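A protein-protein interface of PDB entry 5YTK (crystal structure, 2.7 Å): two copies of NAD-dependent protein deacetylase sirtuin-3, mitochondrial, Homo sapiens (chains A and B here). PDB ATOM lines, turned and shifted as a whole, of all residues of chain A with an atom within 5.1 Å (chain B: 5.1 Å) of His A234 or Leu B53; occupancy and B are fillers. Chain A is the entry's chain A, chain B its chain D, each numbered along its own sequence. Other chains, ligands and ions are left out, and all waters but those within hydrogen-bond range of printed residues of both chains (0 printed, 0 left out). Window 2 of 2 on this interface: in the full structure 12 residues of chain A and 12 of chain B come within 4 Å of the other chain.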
ATOM      1  N   GLU A 212     -39.231 -14.686  -5.181  1.00  0.00           N
ATOM      2  CA  GLU A 212     -39.565 -16.104  -5.200  1.00  0.00           C
ATOM      3  C   GLU A 212     -40.924 -16.371  -4.569  1.00  0.00           C
ATOM      4  O   GLU A 212     -41.339 -17.517  -4.441  1.00  0.00           O
ATOM      5  CB  GLU A 212     -38.488 -16.914  -4.486  1.00  0.00           C
ATOM      6  CG  GLU A 212     -37.113 -16.773  -5.102  1.00  0.00           C
ATOM      7  CD  GLU A 212     -36.110 -17.716  -4.484  1.00  0.00           C
ATOM      8  OE1 GLU A 212     -36.535 -18.637  -3.751  1.00  0.00           O
ATOM      9  OE2 GLU A 212     -34.899 -17.541  -4.736  1.00  0.00           O
ATOM     10  N   ARG A 220     -41.326 -13.896 -14.637  1.00  0.00           N
ATOM     11  CA  ARG A 220     -40.618 -12.800 -14.010  1.00  0.00           C
ATOM     12  C   ARG A 220     -39.799 -12.069 -15.061  1.00  0.00           C
ATOM     13  O   ARG A 220     -38.880 -12.629 -15.641  1.00  0.00           O
ATOM     14  CB  ARG A 220     -39.729 -13.305 -12.874  1.00  0.00           C
ATOM     15  CG  ARG A 220     -40.481 -14.138 -11.853  1.00  0.00           C
ATOM     16  CD  ARG A 220     -39.613 -14.515 -10.686  1.00  0.00           C
ATOM     17  NE  ARG A 220     -38.448 -15.293 -11.089  1.00  0.00           N
ATOM     18  CZ  ARG A 220     -37.570 -15.808 -10.236  1.00  0.00           C
ATOM     19  NH1 ARG A 220     -37.735 -15.641  -8.934  1.00  0.00           N
ATOM     20  NH2 ARG A 220     -36.533 -16.497 -10.683  1.00  0.00           N
ATOM     21  N   GLY A 229     -28.411 -10.843  -8.700  1.00  0.00           N
ATOM     22  CA  GLY A 229     -29.421 -11.024  -7.675  1.00  0.00           C
ATOM     23  C   GLY A 229     -30.118 -12.368  -7.746  1.00  0.00           C
ATOM     24  O   GLY A 229     -29.662 -13.272  -8.445  1.00  0.00           O
ATOM     25  N   PRO A 230     -31.259 -12.490  -7.052  1.00  0.00           N
ATOM     26  CA  PRO A 230     -32.011 -13.742  -6.930  1.00  0.00           C
ATOM     27  C   PRO A 230     -32.460 -14.320  -8.265  1.00  0.00           C
ATOM     28  O   PRO A 230     -32.662 -15.528  -8.360  1.00  0.00           O
ATOM     29  CB  PRO A 230     -33.226 -13.341  -6.091  1.00  0.00           C
ATOM     30  CG  PRO A 230     -32.808 -12.120  -5.372  1.00  0.00           C
ATOM     31  CD  PRO A 230     -31.897 -11.395  -6.304  1.00  0.00           C
ATOM     32  N   LEU A 231     -32.627 -13.481  -9.279  1.00  0.00           N
ATOM     33  CA  LEU A 231     -32.977 -13.998 -10.591  1.00  0.00           C
ATOM     34  C   LEU A 231     -31.760 -14.624 -11.253  1.00  0.00           C
ATOM     35  O   LEU A 231     -31.895 -15.520 -12.080  1.00  0.00           O
ATOM     36  CB  LEU A 231     -33.588 -12.916 -11.489  1.00  0.00           C
ATOM     37  CG  LEU A 231     -35.103 -12.708 -11.346  1.00  0.00           C
ATOM     38  CD1 LEU A 231     -35.465 -11.951 -10.085  1.00  0.00           C
ATOM     39  CD2 LEU A 231     -35.670 -12.011 -12.571  1.00  0.00           C
ATOM     40  N   ALA A 232     -30.569 -14.173 -10.881  1.00  0.00           N
ATOM     41  CA  ALA A 232     -29.355 -14.751 -11.445  1.00  0.00           C
ATOM     42  C   ALA A 232     -29.001 -16.071 -10.772  1.00  0.00           C
ATOM     43  O   ALA A 232     -28.595 -17.014 -11.437  1.00  0.00           O
ATOM     44  CB  ALA A 232     -28.200 -13.777 -11.329  1.00  0.00           C
ATOM     45  N   TRP A 233     -29.153 -16.146  -9.456  1.00  0.00           N
ATOM     46  CA  TRP A 233     -28.773 -17.362  -8.751  1.00  0.00           C
ATOM     47  C   TRP A 233     -29.821 -18.467  -8.887  1.00  0.00           C
ATOM     48  O   TRP A 233     -29.476 -19.629  -9.087  1.00  0.00           O
ATOM     49  CB  TRP A 233     -28.495 -17.071  -7.275  1.00  0.00           C
ATOM     50  CG  TRP A 233     -27.885 -18.241  -6.572  1.00  0.00           C
ATOM     51  CD1 TRP A 233     -28.449 -18.992  -5.586  1.00  0.00           C
ATOM     52  CD2 TRP A 233     -26.607 -18.826  -6.840  1.00  0.00           C
ATOM     53  NE1 TRP A 233     -27.591 -19.992  -5.205  1.00  0.00           N
ATOM     54  CE2 TRP A 233     -26.453 -19.913  -5.964  1.00  0.00           C
ATOM     55  CE3 TRP A 233     -25.571 -18.528  -7.732  1.00  0.00           C
ATOM     56  CZ2 TRP A 233     -25.310 -20.704  -5.951  1.00  0.00           C
ATOM     57  CZ3 TRP A 233     -24.438 -19.313  -7.716  1.00  0.00           C
ATOM     58  CH2 TRP A 233     -24.316 -20.388  -6.832  1.00  0.00           C
ATOM     59  N   HIS A 234     -31.098 -18.107  -8.790  1.00  0.00           N
ATOM     60  CA  HIS A 234     -32.180 -19.088  -8.888  1.00  0.00           C
ATOM     61  C   HIS A 234     -33.146 -18.817 -10.034  1.00  0.00           C
ATOM     62  O   HIS A 234     -34.281 -18.403  -9.796  1.00  0.00           O
ATOM     63  CB  HIS A 234     -32.975 -19.137  -7.583  1.00  0.00           C
ATOM     64  CG  HIS A 234     -32.263 -19.814  -6.457  1.00  0.00           C
ATOM     65  ND1 HIS A 234     -32.469 -19.472  -5.138  1.00  0.00           N
ATOM     66  CD2 HIS A 234     -31.368 -20.831  -6.447  1.00  0.00           C
ATOM     67  CE1 HIS A 234     -31.721 -20.238  -4.364  1.00  0.00           C
ATOM     68  NE2 HIS A 234     -31.043 -21.072  -5.133  1.00  0.00           N
ATOM     69  N   PRO A 235     -32.712 -19.074 -11.277  1.00  0.00           N
ATOM     70  CA  PRO A 235     -33.546 -18.805 -12.449  1.00  0.00           C
ATOM     71  C   PRO A 235     -34.732 -19.748 -12.546  1.00  0.00           C
ATOM     72  O   PRO A 235     -34.664 -20.894 -12.108  1.00  0.00           O
ATOM     73  CB  PRO A 235     -32.592 -19.033 -13.627  1.00  0.00           C
ATOM     74  CG  PRO A 235     -31.229 -19.107 -13.039  1.00  0.00           C
ATOM     75  CD  PRO A 235     -31.415 -19.645 -11.663  1.00  0.00           C
ATOM     76  N   ARG A 236     -35.819 -19.257 -13.116  1.00  0.00           N
ATOM     77  CA  ARG A 236     -36.972 -20.095 -13.371  1.00  0.00           C
ATOM     78  C   ARG A 236     -37.193 -20.140 -14.868  1.00  0.00           C
ATOM     79  O   ARG A 236     -36.673 -19.301 -15.600  1.00  0.00           O
ATOM     80  CB  ARG A 236     -38.199 -19.583 -12.635  1.00  0.00           C
ATOM     81  CG  ARG A 236     -38.056 -19.626 -11.131  1.00  0.00           C
ATOM     82  CD  ARG A 236     -39.312 -19.122 -10.477  1.00  0.00           C
ATOM     83  NE  ARG A 236     -39.257 -19.189  -9.024  1.00  0.00           N
ATOM     84  CZ  ARG A 236     -40.247 -18.794  -8.233  1.00  0.00           C
ATOM     85  NH1 ARG A 236     -41.353 -18.294  -8.759  1.00  0.00           N
ATOM     86  NH2 ARG A 236     -40.129 -18.888  -6.920  1.00  0.00           N
ATOM     87  N   ASP A 239     -38.604 -16.983 -16.742  1.00  0.00           N
ATOM     88  CA  ASP A 239     -37.952 -15.694 -16.500  1.00  0.00           C
ATOM     89  C   ASP A 239     -37.481 -15.063 -17.798  1.00  0.00           C
ATOM     90  O   ASP A 239     -37.040 -15.751 -18.711  1.00  0.00           O
ATOM     91  CB  ASP A 239     -36.765 -15.839 -15.547  1.00  0.00           C
ATOM     92  CG  ASP A 239     -37.189 -16.105 -14.122  1.00  0.00           C
ATOM     93  OD1 ASP A 239     -38.398 -16.051 -13.829  1.00  0.00           O
ATOM     94  OD2 ASP A 239     -36.307 -16.362 -13.286  1.00  0.00           O
ATOM     95  N   LEU B  48     -22.090 -25.012  -9.542  1.00  0.00           N
ATOM     96  CA  LEU B  48     -22.612 -24.631  -8.231  1.00  0.00           C
ATOM     97  C   LEU B  48     -24.129 -24.585  -8.153  1.00  0.00           C
ATOM     98  O   LEU B  48     -24.695 -24.774  -7.080  1.00  0.00           O
ATOM     99  CB  LEU B  48     -22.049 -23.275  -7.800  1.00  0.00           C
ATOM    100  CG  LEU B  48     -20.586 -23.242  -7.361  1.00  0.00           C
ATOM    101  CD1 LEU B  48     -20.188 -21.846  -6.915  1.00  0.00           C
ATOM    102  CD2 LEU B  48     -20.345 -24.251  -6.258  1.00  0.00           C
ATOM    103  N   GLN B  49     -24.797 -24.337  -9.273  1.00  0.00           N
ATOM    104  CA  GLN B  49     -26.259 -24.351  -9.249  1.00  0.00           C
ATOM    105  C   GLN B  49     -26.850 -25.746  -9.049  1.00  0.00           C
ATOM    106  O   GLN B  49     -28.043 -25.880  -8.790  1.00  0.00           O
ATOM    107  CB  GLN B  49     -26.835 -23.718 -10.511  1.00  0.00           C
ATOM    108  CG  GLN B  49     -26.755 -22.212 -10.493  1.00  0.00           C
ATOM    109  CD  GLN B  49     -27.604 -21.583 -11.567  1.00  0.00           C
ATOM    110  OE1 GLN B  49     -28.053 -20.448 -11.427  1.00  0.00           O
ATOM    111  NE2 GLN B  49     -27.829 -22.313 -12.652  1.00  0.00           N
ATOM    112  N   TYR B  51     -26.515 -27.492  -6.625  1.00  0.00           N
ATOM    113  CA  TYR B  51     -26.775 -27.668  -5.196  1.00  0.00           C
ATOM    114  C   TYR B  51     -27.900 -26.763  -4.685  1.00  0.00           C
ATOM    115  O   TYR B  51     -28.388 -25.890  -5.401  1.00  0.00           O
ATOM    116  CB  TYR B  51     -25.500 -27.404  -4.386  1.00  0.00           C
ATOM    117  CG  TYR B  51     -24.296 -28.220  -4.821  1.00  0.00           C
ATOM    118  CD1 TYR B  51     -24.099 -29.513  -4.356  1.00  0.00           C
ATOM    119  CD2 TYR B  51     -23.346 -27.686  -5.682  1.00  0.00           C
ATOM    120  CE1 TYR B  51     -22.998 -30.255  -4.750  1.00  0.00           C
ATOM    121  CE2 TYR B  51     -22.244 -28.420  -6.076  1.00  0.00           C
ATOM    122  CZ  TYR B  51     -22.074 -29.703  -5.608  1.00  0.00           C
ATOM    123  OH  TYR B  51     -20.977 -30.432  -6.001  1.00  0.00           O
ATOM    124  N   ASP B  52     -28.296 -26.979  -3.434  1.00  0.00           N
ATOM    125  CA  ASP B  52     -29.395 -26.241  -2.816  1.00  0.00           C
ATOM    126  C   ASP B  52     -28.951 -24.938  -2.143  1.00  0.00           C
ATOM    127  O   ASP B  52     -29.360 -24.648  -1.020  1.00  0.00           O
ATOM    128  CB  ASP B  52     -30.112 -27.130  -1.792  1.00  0.00           C
ATOM    129  CG  ASP B  52     -29.199 -27.579  -0.659  1.00  0.00           C
ATOM    130  OD1 ASP B  52     -28.255 -28.356  -0.919  1.00  0.00           O
ATOM    131  OD2 ASP B  52     -29.429 -27.160   0.495  1.00  0.00           O
ATOM    132  N   LEU B  53     -28.126 -24.148  -2.823  1.00  0.00           N
ATOM    133  CA  LEU B  53     -27.678 -22.876  -2.260  1.00  0.00           C
ATOM    134  C   LEU B  53     -28.715 -21.782  -2.418  1.00  0.00           C
ATOM    135  O   LEU B  53     -29.174 -21.521  -3.521  1.00  0.00           O
ATOM    136  CB  LEU B  53     -26.367 -22.431  -2.914  1.00  0.00           C
ATOM    137  CG  LEU B  53     -25.091 -23.192  -2.561  1.00  0.00           C
ATOM    138  CD1 LEU B  53     -24.023 -22.959  -3.601  1.00  0.00           C
ATOM    139  CD2 LEU B  53     -24.602 -22.700  -1.221  1.00  0.00           C
ATOM    140  N   PRO B  54     -29.065 -21.115  -1.309  1.00  0.00           N
ATOM    141  CA  PRO B  54     -30.020 -20.003  -1.315  1.00  0.00           C
ATOM    142  C   PRO B  54     -29.437 -18.729  -1.924  1.00  0.00           C
ATOM    143  O   PRO B  54     -30.173 -17.908  -2.467  1.00  0.00           O
ATOM    144  CB  PRO B  54     -30.332 -19.807   0.169  1.00  0.00           C
ATOM    145  CG  PRO B  54     -29.116 -20.297   0.873  1.00  0.00           C
ATOM    146  CD  PRO B  54     -28.604 -21.441   0.050  1.00  0.00           C
ATOM    147  N   TYR B  55     -28.124 -18.579  -1.817  1.00  0.00           N
ATOM    148  CA  TYR B  55     -27.399 -17.445  -2.370  1.00  0.00           C
ATOM    149  C   TYR B  55     -25.915 -17.817  -2.382  1.00  0.00           C
ATOM    150  O   TYR B  55     -25.503 -18.694  -1.628  1.00  0.00           O
ATOM    151  CB  TYR B  55     -27.665 -16.181  -1.550  1.00  0.00           C
ATOM    152  CG  TYR B  55     -27.637 -16.401  -0.056  1.00  0.00           C
ATOM    153  CD1 TYR B  55     -26.437 -16.400   0.642  1.00  0.00           C
ATOM    154  CD2 TYR B  55     -28.808 -16.606   0.661  1.00  0.00           C
ATOM    155  CE1 TYR B  55     -26.405 -16.604   2.008  1.00  0.00           C
ATOM    156  CE2 TYR B  55     -28.785 -16.809   2.028  1.00  0.00           C
ATOM    157  CZ  TYR B  55     -27.580 -16.806   2.695  1.00  0.00           C
ATOM    158  OH  TYR B  55     -27.541 -17.008   4.056  1.00  0.00           O
ATOM    159  N   PRO B  56     -25.112 -17.171  -3.249  1.00  0.00           N
ATOM    160  CA  PRO B  56     -23.690 -17.520  -3.386  1.00  0.00           C
ATOM    161  C   PRO B  56     -22.905 -17.482  -2.072  1.00  0.00           C
ATOM    162  O   PRO B  56     -22.114 -18.386  -1.812  1.00  0.00           O
ATOM    163  CB  PRO B  56     -23.163 -16.455  -4.350  1.00  0.00           C
ATOM    164  CG  PRO B  56     -24.339 -16.044  -5.136  1.00  0.00           C
ATOM    165  CD  PRO B  56     -25.521 -16.147  -4.225  1.00  0.00           C
ATOM    166  N   ALA B  58     -23.549 -18.253   0.747  1.00  0.00           N
ATOM    167  CA  ALA B  58     -23.782 -19.422   1.592  1.00  0.00           C
ATOM    168  C   ALA B  58     -22.679 -20.453   1.419  1.00  0.00           C
ATOM    169  O   ALA B  58     -22.565 -21.387   2.204  1.00  0.00           O
ATOM    170  CB  ALA B  58     -25.128 -20.040   1.291  1.00  0.00           C
ATOM    171  N   ILE B  59     -21.876 -20.295   0.379  1.00  0.00           N
ATOM    172  CA  ILE B  59     -20.758 -21.194   0.172  1.00  0.00           C
ATOM    173  C   ILE B  59     -19.677 -20.939   1.221  1.00  0.00           C
ATOM    174  O   ILE B  59     -18.858 -21.809   1.504  1.00  0.00           O
ATOM    175  CB  ILE B  59     -20.182 -21.031  -1.249  1.00  0.00           C
ATOM    176  CG1 ILE B  59     -19.449 -22.289  -1.689  1.00  0.00           C
ATOM    177  CG2 ILE B  59     -19.267 -19.827  -1.342  1.00  0.00           C
ATOM    178  CD1 ILE B  59     -19.036 -22.238  -3.135  1.00  0.00           C
ATOM    179  N   PHE B  64     -24.121 -24.146   6.407  1.00  0.00           N
ATOM    180  CA  PHE B  64     -24.312 -24.811   5.135  1.00  0.00           C
ATOM    181  C   PHE B  64     -23.190 -25.794   4.853  1.00  0.00           C
ATOM    182  O   PHE B  64     -23.429 -26.878   4.329  1.00  0.00           O
ATOM    183  CB  PHE B  64     -24.399 -23.802   3.993  1.00  0.00           C
ATOM    184  CG  PHE B  64     -24.881 -24.407   2.715  1.00  0.00           C
ATOM    185  CD1 PHE B  64     -24.001 -25.057   1.861  1.00  0.00           C
ATOM    186  CD2 PHE B  64     -26.224 -24.370   2.385  1.00  0.00           C
ATOM    187  CE1 PHE B  64     -24.448 -25.639   0.694  1.00  0.00           C
ATOM    188  CE2 PHE B  64     -26.675 -24.948   1.218  1.00  0.00           C
ATOM    189  CZ  PHE B  64     -25.786 -25.584   0.371  1.00  0.00           C
ATOM    190  N   PRO B  71     -20.425 -28.013  -2.191  1.00  0.00           N
ATOM    191  CA  PRO B  71     -20.282 -26.784  -2.982  1.00  0.00           C
ATOM    192  C   PRO B  71     -18.975 -26.037  -2.739  1.00  0.00           C
ATOM    193  O   PRO B  71     -18.260 -25.664  -3.689  1.00  0.00           O
ATOM    194  CB  PRO B  71     -21.470 -25.943  -2.521  1.00  0.00           C
ATOM    195  CG  PRO B  71     -22.481 -26.927  -2.117  1.00  0.00           C
ATOM    196  CD  PRO B  71     -21.725 -28.052  -1.494  1.00  0.00           C
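Among the printed residues, pairs that only touch across the chains: His A234 with Pro B54 (3.4 Å), Pro A235 with Gln B49 (3.5 Å), Trp A233 with Tyr B55 (3.7 Å), Trp A233 with Pro B54 (3.7 Å), Trp A233 with Leu B48 (3.8 Å) and Trp A233 with Pro B56 (3.8 Å).
Of the printed residues of chain B, Ala A232 touches Gln B49 (3.5 Å). Of the printed residues of chain B, Trp A233 touches Leu B48, Gln B49, Leu B53, Pro B54, Tyr B55 and Pro B56. Of chain B, only Leu B53 (2.5 Å) and Pro B54 (3.4 Å) come within 4 Å of His A234. Of chain A, only Trp A233 (2.8 Å) and His A234 (2.5 Å) come within 4 Å of Leu B53. The nearest residue of chain B that does not touch His A234 is Gln B49 (4.7 Å). The nearest printed residue of chain A that does not touch Leu B53 is Glu A212 (7.1 Å).
No position is printed for both chains. Of the 10 pairs that touch across the chains among the printed residues, none has its exchanged pair printed and touching as well.
A ring nitrogen (ND1) of His A234 sits at hydrogen-bond distance from the side-chain carboxylate (OE2) of Glu A212 (3.1 Å). The backbone carbonyl oxygen (O) of His A234 lies within hydrogen-bond range of the guanidinium group (NH2) of Arg A220 (3.1 Å).
Of the 12 printed residues of chain B, 6 touch a printed residue of chain A. Hydrophobic or aromatic side chains of chain A within 4 Å of the printed part of chain B: Trp A233, His A234 and Pro A235. Among the printed residues, 10 pairs touch across the chains.
O of Ala A232 lies close to OE1 of Gln B49 (3.5 Å). The side-chain amide oxygen of Gln B49 lies close to the backbone carbonyl oxygen of Trp A233 (2.9 Å). The indole nitrogen (NE1) of Trp A233 is in hydrogen-bond range of the backbone carbonyl oxygen (O) of Leu B53, 2.8 Å away. The backbone carbonyl oxygen of Leu B53 lies within hydrogen-bond range of a ring nitrogen (NE2) of His A234, at 2.5 Å.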
